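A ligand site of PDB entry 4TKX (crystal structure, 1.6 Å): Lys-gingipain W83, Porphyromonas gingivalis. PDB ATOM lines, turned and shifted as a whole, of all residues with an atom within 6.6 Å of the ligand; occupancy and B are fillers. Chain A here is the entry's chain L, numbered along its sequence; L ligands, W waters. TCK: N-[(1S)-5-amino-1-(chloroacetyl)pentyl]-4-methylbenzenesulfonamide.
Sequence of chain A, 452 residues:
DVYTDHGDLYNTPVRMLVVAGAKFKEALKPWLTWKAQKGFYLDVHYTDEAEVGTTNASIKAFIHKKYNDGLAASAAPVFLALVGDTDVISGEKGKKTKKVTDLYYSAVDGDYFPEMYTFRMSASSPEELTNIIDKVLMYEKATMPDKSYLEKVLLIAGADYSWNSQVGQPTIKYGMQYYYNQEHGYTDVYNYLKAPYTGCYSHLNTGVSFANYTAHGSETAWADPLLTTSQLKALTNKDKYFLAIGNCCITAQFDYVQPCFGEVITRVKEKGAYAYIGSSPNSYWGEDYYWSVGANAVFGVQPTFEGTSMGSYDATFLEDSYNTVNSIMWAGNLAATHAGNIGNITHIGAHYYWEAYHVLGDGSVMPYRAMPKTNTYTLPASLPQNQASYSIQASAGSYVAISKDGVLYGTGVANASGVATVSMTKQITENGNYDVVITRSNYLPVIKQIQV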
ATOM      1  N   ASP A 160      -0.870  -0.006  28.633  1.00  0.00           N
ATOM      2  CA  ASP A 160      -2.228  -0.256  29.045  1.00  0.00           C
ATOM      3  C   ASP A 160      -2.677  -1.471  28.247  1.00  0.00           C
ATOM      4  O   ASP A 160      -2.753  -1.419  27.015  1.00  0.00           O
ATOM      5  CB  ASP A 160      -3.140   0.936  28.785  1.00  0.00           C
ATOM      6  CG  ASP A 160      -4.527   0.707  29.337  1.00  0.00           C
ATOM      7  OD1 ASP A 160      -5.184  -0.228  28.810  1.00  0.00           O
ATOM      8  OD2 ASP A 160      -4.939   1.420  30.279  1.00  0.00           O
ATOM      9  N   TRP A 163      -5.730  -0.263  26.013  1.00  0.00           N
ATOM     10  CA  TRP A 163      -5.772   0.993  25.270  1.00  0.00           C
ATOM     11  C   TRP A 163      -4.502   1.258  24.469  1.00  0.00           C
ATOM     12  O   TRP A 163      -4.489   2.095  23.552  1.00  0.00           O
ATOM     13  CB  TRP A 163      -5.977   2.156  26.227  1.00  0.00           C
ATOM     14  CG  TRP A 163      -7.368   2.295  26.739  1.00  0.00           C
ATOM     15  CD1 TRP A 163      -7.831   2.010  27.990  1.00  0.00           C
ATOM     16  CD2 TRP A 163      -8.481   2.790  26.001  1.00  0.00           C
ATOM     17  NE1 TRP A 163      -9.171   2.292  28.074  1.00  0.00           N
ATOM     18  CE2 TRP A 163      -9.591   2.775  26.862  1.00  0.00           C
ATOM     19  CE3 TRP A 163      -8.643   3.238  24.691  1.00  0.00           C
ATOM     20  CZ2 TRP A 163     -10.851   3.187  26.450  1.00  0.00           C
ATOM     21  CZ3 TRP A 163      -9.889   3.652  24.292  1.00  0.00           C
ATOM     22  CH2 TRP A 163     -10.974   3.624  25.161  1.00  0.00           C
ATOM     23  N   VAL A 167      -5.385   3.036  20.931  1.00  0.00           N
ATOM     24  CA  VAL A 167      -5.224   4.487  20.865  1.00  0.00           C
ATOM     25  C   VAL A 167      -3.764   4.924  20.947  1.00  0.00           C
ATOM     26  O   VAL A 167      -3.318   5.773  20.164  1.00  0.00           O
ATOM     27  CB  VAL A 167      -6.044   5.163  21.971  1.00  0.00           C
ATOM     28  CG1 VAL A 167      -5.648   6.633  22.109  1.00  0.00           C
ATOM     29  CG2 VAL A 167      -7.549   5.010  21.691  1.00  0.00           C
ATOM     30  N   TYR A 213       4.842  11.262  25.669  1.00  0.00           N
ATOM     31  CA  TYR A 213       4.353  10.045  26.311  1.00  0.00           C
ATOM     32  C   TYR A 213       2.833  10.095  26.352  1.00  0.00           C
ATOM     33  O   TYR A 213       2.261  11.106  26.732  1.00  0.00           O
ATOM     34  CB  TYR A 213       4.911   9.972  27.733  1.00  0.00           C
ATOM     35  CG  TYR A 213       4.289   8.951  28.658  1.00  0.00           C
ATOM     36  CD1 TYR A 213       3.151   9.255  29.383  1.00  0.00           C
ATOM     37  CD2 TYR A 213       4.871   7.696  28.849  1.00  0.00           C
ATOM     38  CE1 TYR A 213       2.596   8.333  30.264  1.00  0.00           C
ATOM     39  CE2 TYR A 213       4.304   6.767  29.730  1.00  0.00           C
ATOM     40  CZ  TYR A 213       3.160   7.098  30.413  1.00  0.00           C
ATOM     41  OH  TYR A 213       2.612   6.191  31.298  1.00  0.00           O
ATOM     42  N   THR A 214       2.196   9.010  25.906  1.00  0.00           N
ATOM     43  CA  THR A 214       0.759   8.875  26.029  1.00  0.00           C
ATOM     44  C   THR A 214       0.396   7.518  26.657  1.00  0.00           C
ATOM     45  O   THR A 214       0.728   6.453  26.113  1.00  0.00           O
ATOM     46  CB  THR A 214       0.036   9.092  24.675  1.00  0.00           C
ATOM     47  OG1 THR A 214      -1.352   8.869  24.866  1.00  0.00           O
ATOM     48  CG2 THR A 214       0.548   8.130  23.580  1.00  0.00           C
ATOM     49  N   ALA A 215      -0.228   7.616  27.837  1.00  0.00           N
ATOM     50  CA  ALA A 215      -0.722   6.476  28.641  1.00  0.00           C
ATOM     51  C   ALA A 215      -0.974   7.033  30.056  1.00  0.00           C
ATOM     52  O   ALA A 215      -1.455   8.150  30.179  1.00  0.00           O
ATOM     53  CB  ALA A 215       0.226   5.328  28.654  1.00  0.00           C
ATOM     54  N   HIS A 216      -0.714   6.266  31.113  1.00  0.00           N
ATOM     55  CA  HIS A 216      -1.130   6.706  32.445  1.00  0.00           C
ATOM     56  C   HIS A 216      -0.126   7.614  33.129  1.00  0.00           C
ATOM     57  O   HIS A 216       1.082   7.445  32.997  1.00  0.00           O
ATOM     58  CB  HIS A 216      -1.377   5.490  33.345  1.00  0.00           C
ATOM     59  CG  HIS A 216      -2.522   4.631  32.896  1.00  0.00           C
ATOM     60  ND1 HIS A 216      -3.769   4.703  33.476  1.00  0.00           N
ATOM     61  CD2 HIS A 216      -2.594   3.666  31.951  1.00  0.00           C
ATOM     62  CE1 HIS A 216      -4.580   3.836  32.890  1.00  0.00           C
ATOM     63  NE2 HIS A 216      -3.886   3.190  31.966  1.00  0.00           N
ATOM     64  N   GLY A 217      -0.646   8.560  33.902  1.00  0.00           N
ATOM     65  CA  GLY A 217       0.184   9.477  34.661  1.00  0.00           C
ATOM     66  C   GLY A 217      -0.297   9.674  36.079  1.00  0.00           C
ATOM     67  O   GLY A 217      -1.452   9.367  36.424  1.00  0.00           O
ATOM     68  N   SER A 218       0.584  10.211  36.918  1.00  0.00           N
ATOM     69  CA  SER A 218       0.209  10.636  38.254  1.00  0.00           C
ATOM     70  C   SER A 218       0.802  12.020  38.469  1.00  0.00           C
ATOM     71  O   SER A 218       1.438  12.577  37.564  1.00  0.00           O
ATOM     72  CB  SER A 218       0.780   9.670  39.294  1.00  0.00           C
ATOM     73  OG  SER A 218       2.165   9.888  39.395  1.00  0.00           O
ATOM     74  N   ASN A 247       0.668  13.364  27.516  1.00  0.00           N
ATOM     75  CA  ASN A 247      -0.753  13.207  27.252  1.00  0.00           C
ATOM     76  C   ASN A 247      -1.222  12.110  28.195  1.00  0.00           C
ATOM     77  O   ASN A 247      -1.224  10.923  27.858  1.00  0.00           O
ATOM     78  CB  ASN A 247      -0.983  12.837  25.786  1.00  0.00           C
ATOM     79  CG  ASN A 247      -0.640  13.965  24.850  1.00  0.00           C
ATOM     80  OD1 ASN A 247       0.246  13.842  24.014  1.00  0.00           O
ATOM     81  ND2 ASN A 247      -1.315  15.097  25.008  1.00  0.00           N
ATOM     82  N   CYS A 248      -1.554  12.531  29.402  1.00  0.00           N
ATOM     83  CA  CYS A 248      -1.882  11.613  30.484  1.00  0.00           C
ATOM     84  C   CYS A 248      -2.486  12.419  31.630  1.00  0.00           C
ATOM     85  O   CYS A 248      -2.525  13.641  31.570  1.00  0.00           O
ATOM     86  CB  CYS A 248      -0.623  10.883  30.961  1.00  0.00           C
ATOM     87  SG  CYS A 248       0.724  11.931  31.526  1.00  0.00           S
ATOM     88  N   CYS A 249      -2.934  11.731  32.673  1.00  0.00           N
ATOM     89  CA  CYS A 249      -3.480  12.426  33.841  1.00  0.00           C
ATOM     90  C   CYS A 249      -2.459  13.215  34.647  1.00  0.00           C
ATOM     91  O   CYS A 249      -1.333  12.785  34.824  1.00  0.00           O
ATOM     92  CB  CYS A 249      -4.126  11.431  34.786  1.00  0.00           C
ATOM     93  SG  CYS A 249      -5.540  10.574  34.063  1.00  0.00           S
ATOM     94  N   ILE A 250      -2.934  14.360  35.119  1.00  0.00           N
ATOM     95  CA  ILE A 250      -2.461  15.105  36.304  1.00  0.00           C
ATOM     96  C   ILE A 250      -0.966  15.473  36.508  1.00  0.00           C
ATOM     97  O   ILE A 250      -0.607  16.037  37.544  1.00  0.00           O
ATOM     98  CB  ILE A 250      -3.016  14.486  37.644  1.00  0.00           C
ATOM     99  CG1 ILE A 250      -2.429  13.091  37.930  1.00  0.00           C
ATOM    100  CG2 ILE A 250      -4.570  14.448  37.607  1.00  0.00           C
ATOM    101  CD1 ILE A 250      -2.996  12.444  39.201  1.00  0.00           C
ATOM    102  N   ASN A 282      -7.438  14.832  35.335  1.00  0.00           N
ATOM    103  CA  ASN A 282      -7.375  13.646  34.512  1.00  0.00           C
ATOM    104  C   ASN A 282      -7.512  13.971  33.028  1.00  0.00           C
ATOM    105  O   ASN A 282      -8.206  14.908  32.655  1.00  0.00           O
ATOM    106  CB  ASN A 282      -8.514  12.694  34.885  1.00  0.00           C
ATOM    107  CG  ASN A 282      -8.384  12.154  36.273  1.00  0.00           C
ATOM    108  OD1 ASN A 282      -7.296  12.099  36.834  1.00  0.00           O
ATOM    109  ND2 ASN A 282      -9.506  11.719  36.842  1.00  0.00           N
ATOM    110  N   SER A 283      -6.820  13.212  32.187  1.00  0.00           N
ATOM    111  CA  SER A 283      -7.084  13.224  30.751  1.00  0.00           C
ATOM    112  C   SER A 283      -7.696  11.872  30.377  1.00  0.00           C
ATOM    113  O   SER A 283      -7.742  10.934  31.189  1.00  0.00           O
ATOM    114  CB  SER A 283      -5.823  13.519  29.924  1.00  0.00           C
ATOM    115  OG  SER A 283      -4.976  12.396  29.848  1.00  0.00           O
ATOM    116  N   TYR A 284      -8.181  11.781  29.145  1.00  0.00           N
ATOM    117  CA  TYR A 284      -8.964  10.622  28.719  1.00  0.00           C
ATOM    118  C   TYR A 284      -8.475  10.144  27.378  1.00  0.00           C
ATOM    119  O   TYR A 284      -7.925  10.915  26.604  1.00  0.00           O
ATOM    120  CB  TYR A 284     -10.444  10.968  28.658  1.00  0.00           C
ATOM    121  CG  TYR A 284     -10.960  11.284  30.016  1.00  0.00           C
ATOM    122  CD1 TYR A 284     -11.344  10.272  30.886  1.00  0.00           C
ATOM    123  CD2 TYR A 284     -10.991  12.584  30.480  1.00  0.00           C
ATOM    124  CE1 TYR A 284     -11.793  10.549  32.167  1.00  0.00           C
ATOM    125  CE2 TYR A 284     -11.439  12.889  31.756  1.00  0.00           C
ATOM    126  CZ  TYR A 284     -11.830  11.863  32.591  1.00  0.00           C
ATOM    127  OH  TYR A 284     -12.261  12.168  33.865  1.00  0.00           O
ATOM    128  N   TRP A 285      -8.646   8.875  27.099  1.00  0.00           N
ATOM    129  CA  TRP A 285      -8.078   8.310  25.897  1.00  0.00           C
ATOM    130  C   TRP A 285      -8.600   8.956  24.597  1.00  0.00           C
ATOM    131  O   TRP A 285      -7.808   9.308  23.719  1.00  0.00           O
ATOM    132  CB  TRP A 285      -8.251   6.791  25.873  1.00  0.00           C
ATOM    133  CG  TRP A 285      -7.423   6.084  26.916  1.00  0.00           C
ATOM    134  CD1 TRP A 285      -7.852   5.661  28.159  1.00  0.00           C
ATOM    135  CD2 TRP A 285      -6.049   5.691  26.818  1.00  0.00           C
ATOM    136  NE1 TRP A 285      -6.815   5.049  28.825  1.00  0.00           N
ATOM    137  CE2 TRP A 285      -5.707   5.048  28.026  1.00  0.00           C
ATOM    138  CE3 TRP A 285      -5.067   5.832  25.831  1.00  0.00           C
ATOM    139  CZ2 TRP A 285      -4.421   4.543  28.259  1.00  0.00           C
ATOM    140  CZ3 TRP A 285      -3.799   5.313  26.069  1.00  0.00           C
ATOM    141  CH2 TRP A 285      -3.485   4.678  27.277  1.00  0.00           C
ATOM    142  N   GLY A 286      -9.912   9.127  24.489  1.00  0.00           N
ATOM    143  CA  GLY A 286     -10.479   9.664  23.257  1.00  0.00           C
ATOM    144  C   GLY A 286     -10.051  11.097  23.038  1.00  0.00           C
ATOM    145  O   GLY A 286      -9.584  11.469  21.968  1.00  0.00           O
ATOM    146  N   ASP A 288      -7.477  12.756  24.249  1.00  0.00           N
ATOM    147  CA  ASP A 288      -6.032  12.908  23.956  1.00  0.00           C
ATOM    148  C   ASP A 288      -5.710  12.413  22.529  1.00  0.00           C
ATOM    149  O   ASP A 288      -4.795  12.883  21.876  1.00  0.00           O
ATOM    150  CB  ASP A 288      -5.164  12.139  24.941  1.00  0.00           C
ATOM    151  CG  ASP A 288      -4.955  12.857  26.272  1.00  0.00           C
ATOM    152  OD1 ASP A 288      -5.426  14.007  26.450  1.00  0.00           O
ATOM    153  OD2 ASP A 288      -4.287  12.252  27.140  1.00  0.00           O
ATOM    154  N   TYR A 289      -6.471  11.426  22.060  1.00  0.00           N
ATOM    155  CA  TYR A 289      -6.284  10.875  20.711  1.00  0.00           C
ATOM    156  C   TYR A 289      -6.551  11.992  19.706  1.00  0.00           C
ATOM    157  O   TYR A 289      -5.718  12.262  18.816  1.00  0.00           O
ATOM    158  CB  TYR A 289      -7.273   9.736  20.520  1.00  0.00           C
ATOM    159  CG  TYR A 289      -7.129   8.790  19.322  1.00  0.00           C
ATOM    160  CD1 TYR A 289      -5.953   8.669  18.608  1.00  0.00           C
ATOM    161  CD2 TYR A 289      -8.201   7.982  18.947  1.00  0.00           C
ATOM    162  CE1 TYR A 289      -5.842   7.781  17.547  1.00  0.00           C
ATOM    163  CE2 TYR A 289      -8.095   7.102  17.890  1.00  0.00           C
ATOM    164  CZ  TYR A 289      -6.922   6.998  17.190  1.00  0.00           C
ATOM    165  OH  TYR A 289      -6.828   6.096  16.135  1.00  0.00           O
ATOM    166  N   TYR A 353     -11.136  20.630  28.424  1.00  0.00           N
ATOM    167  CA  TYR A 353      -9.788  20.537  27.890  1.00  0.00           C
ATOM    168  C   TYR A 353      -9.062  21.865  27.936  1.00  0.00           C
ATOM    169  O   TYR A 353      -7.858  21.912  28.257  1.00  0.00           O
ATOM    170  CB  TYR A 353      -9.765  19.933  26.487  1.00  0.00           C
ATOM    171  CG  TYR A 353      -9.343  18.484  26.606  1.00  0.00           C
ATOM    172  CD1 TYR A 353     -10.070  17.608  27.394  1.00  0.00           C
ATOM    173  CD2 TYR A 353      -8.179  18.017  26.002  1.00  0.00           C
ATOM    174  CE1 TYR A 353      -9.679  16.301  27.574  1.00  0.00           C
ATOM    175  CE2 TYR A 353      -7.787  16.698  26.156  1.00  0.00           C
ATOM    176  CZ  TYR A 353      -8.544  15.856  26.967  1.00  0.00           C
ATOM    177  OH  TYR A 353      -8.202  14.547  27.140  1.00  0.00           O
ATOM    178  N   TYR A 357      -5.320  21.521  30.102  1.00  0.00           N
ATOM    179  CA  TYR A 357      -3.951  21.529  29.598  1.00  0.00           C
ATOM    180  C   TYR A 357      -3.242  22.849  29.894  1.00  0.00           C
ATOM    181  O   TYR A 357      -3.817  23.934  29.787  1.00  0.00           O
ATOM    182  CB  TYR A 357      -3.917  21.159  28.107  1.00  0.00           C
ATOM    183  CG  TYR A 357      -3.795  19.676  27.876  1.00  0.00           C
ATOM    184  CD1 TYR A 357      -2.554  19.063  27.830  1.00  0.00           C
ATOM    185  CD2 TYR A 357      -4.915  18.886  27.735  1.00  0.00           C
ATOM    186  CE1 TYR A 357      -2.434  17.701  27.634  1.00  0.00           C
ATOM    187  CE2 TYR A 357      -4.798  17.506  27.517  1.00  0.00           C
ATOM    188  CZ  TYR A 357      -3.556  16.930  27.476  1.00  0.00           C
ATOM    189  OH  TYR A 357      -3.399  15.577  27.284  1.00  0.00           O
HETATM  190  S   TCK L   1      -7.867   7.226  32.434  1.00  0.00           S
HETATM  191  O1S TCK L   1      -8.667   7.325  31.240  1.00  0.00           O
HETATM  192  O2S TCK L   1      -7.250   5.903  32.431  1.00  0.00           O
HETATM  193  C1  TCK L   1      -8.874   7.414  33.900  1.00  0.00           C
HETATM  194  C2  TCK L   1      -8.953   6.346  34.786  1.00  0.00           C
HETATM  195  C3  TCK L   1      -9.737   6.479  35.949  1.00  0.00           C
HETATM  196  C4  TCK L   1     -10.409   7.655  36.183  1.00  0.00           C
HETATM  197  C5  TCK L   1     -10.327   8.732  35.277  1.00  0.00           C
HETATM  198  C6  TCK L   1      -9.558   8.610  34.127  1.00  0.00           C
HETATM  199  C7  TCK L   1     -11.256   7.775  37.427  1.00  0.00           C
HETATM  200  N   TCK L   1      -6.726   8.421  32.401  1.00  0.00           N
HETATM  201  CA  TCK L   1      -5.300   8.157  32.196  1.00  0.00           C
HETATM  202  C   TCK L   1      -4.547   8.713  33.380  1.00  0.00           C
HETATM  203  O   TCK L   1      -3.383   9.011  33.301  1.00  0.00           O
HETATM  204  CB  TCK L   1      -4.817   8.865  30.898  1.00  0.00           C
HETATM  205  CG  TCK L   1      -5.434   8.239  29.663  1.00  0.00           C
HETATM  206  CD  TCK L   1      -5.119   9.061  28.354  1.00  0.00           C
HETATM  207  CE  TCK L   1      -3.760   8.774  27.789  1.00  0.00           C
HETATM  208  NZ  TCK L   1      -3.524   9.605  26.632  1.00  0.00           N
HETATM  209  CM  TCK L   1      -5.345   8.967  34.677  1.00  0.00           C
HETATM  210  O   HOH W   1      -7.985   3.850  31.269  1.00  0.00           O
HETATM  211  O   HOH W   2     -11.255   6.247  30.404  1.00  0.00           O
HETATM  212  O   HOH W   3      -5.033   8.922  24.283  1.00  0.00           O
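The side-chain hydroxyl (OG1) of Thr 214 lies within hydrogen-bond range of a nitrogen (NZ) of the ligand.
The backbone NH (N) of Gly 217 is in hydrogen-bond range of an oxygen (O) of the ligand (2.8 Å).
The side-chain sulfur (SG) of Cys 249 is bonded to a carbon (CM) of the ligand (1.7 Å).
A nitrogen (NZ) of the ligand lies within hydrogen-bond range of the backbone carbonyl oxygen of Asn 247, at 2.9 Å.
An oxygen (O) of the ligand lies within hydrogen-bond range of the backbone NH (N) of Cys 249, 2.8 Å away.
A nitrogen (N) of the ligand sits at hydrogen-bond distance from the backbone carbonyl oxygen of Ser 283, at 3.0 Å.
The side-chain carboxylate of Asp 288 lies within salt-bridge range of a nitrogen (NZ) of the ligand (2.8 Å).
The side-chain carboxylate (OD1) of Asp 288 lies within hydrogen-bond range of the side-chain hydroxyl (OH) of Tyr 357, at 2.7 Å.
SG of Cys 249 sits at hydrogen-bond distance from N of Ser 283 (3.5 Å).
The backbone NH (N) of Tyr 284 sits at hydrogen-bond distance from the side-chain hydroxyl (OH) of Tyr 353, 3.4 Å away.
O of Asn 247 sits at hydrogen-bond distance from N of Ala 215, at 3.5 Å.
NE2 of His 216 is in hydrogen-bond range of OD2 of Asp 160 (2.7 Å).
The side-chain hydroxyl (OH) of Tyr 213 lies within hydrogen-bond range of the backbone carbonyl oxygen (O) of His 216 (2.6 Å).
The side-chain amide oxygen (OD1) of Asn 282 lies close to the side-chain sulfur (SG) of Cys 249, 3.6 Å away.
The side-chain hydroxyl (OH) of Tyr 353 sits at hydrogen-bond distance from the side-chain carboxylate (OD1) of Asp 288 (2.9 Å).
Residues that only touch the ligand: Ala 215 (3.4 Å), His 216 (3.3 Å), Cys 248 (3.9 Å), Asn 282 (3.5 Å), Tyr 284 (3.5 Å) and Trp 285 (3.6 Å).
Hydrophobic or aromatic side chains within 4 Å of the ligand: His 216, Tyr 284 and Trp 285.
Of the 22 residues printed, 12 come within 4 Å of the ligand.
Water W1 lies within hydrogen-bond range of an oxygen (O2S) of the ligand and the indole nitrogen of Trp 285.
Water W3 bridges the backbone carbonyl oxygen (O) of Trp 285 (2.9 Å) and a nitrogen (NZ) of the ligand (2.9 Å).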
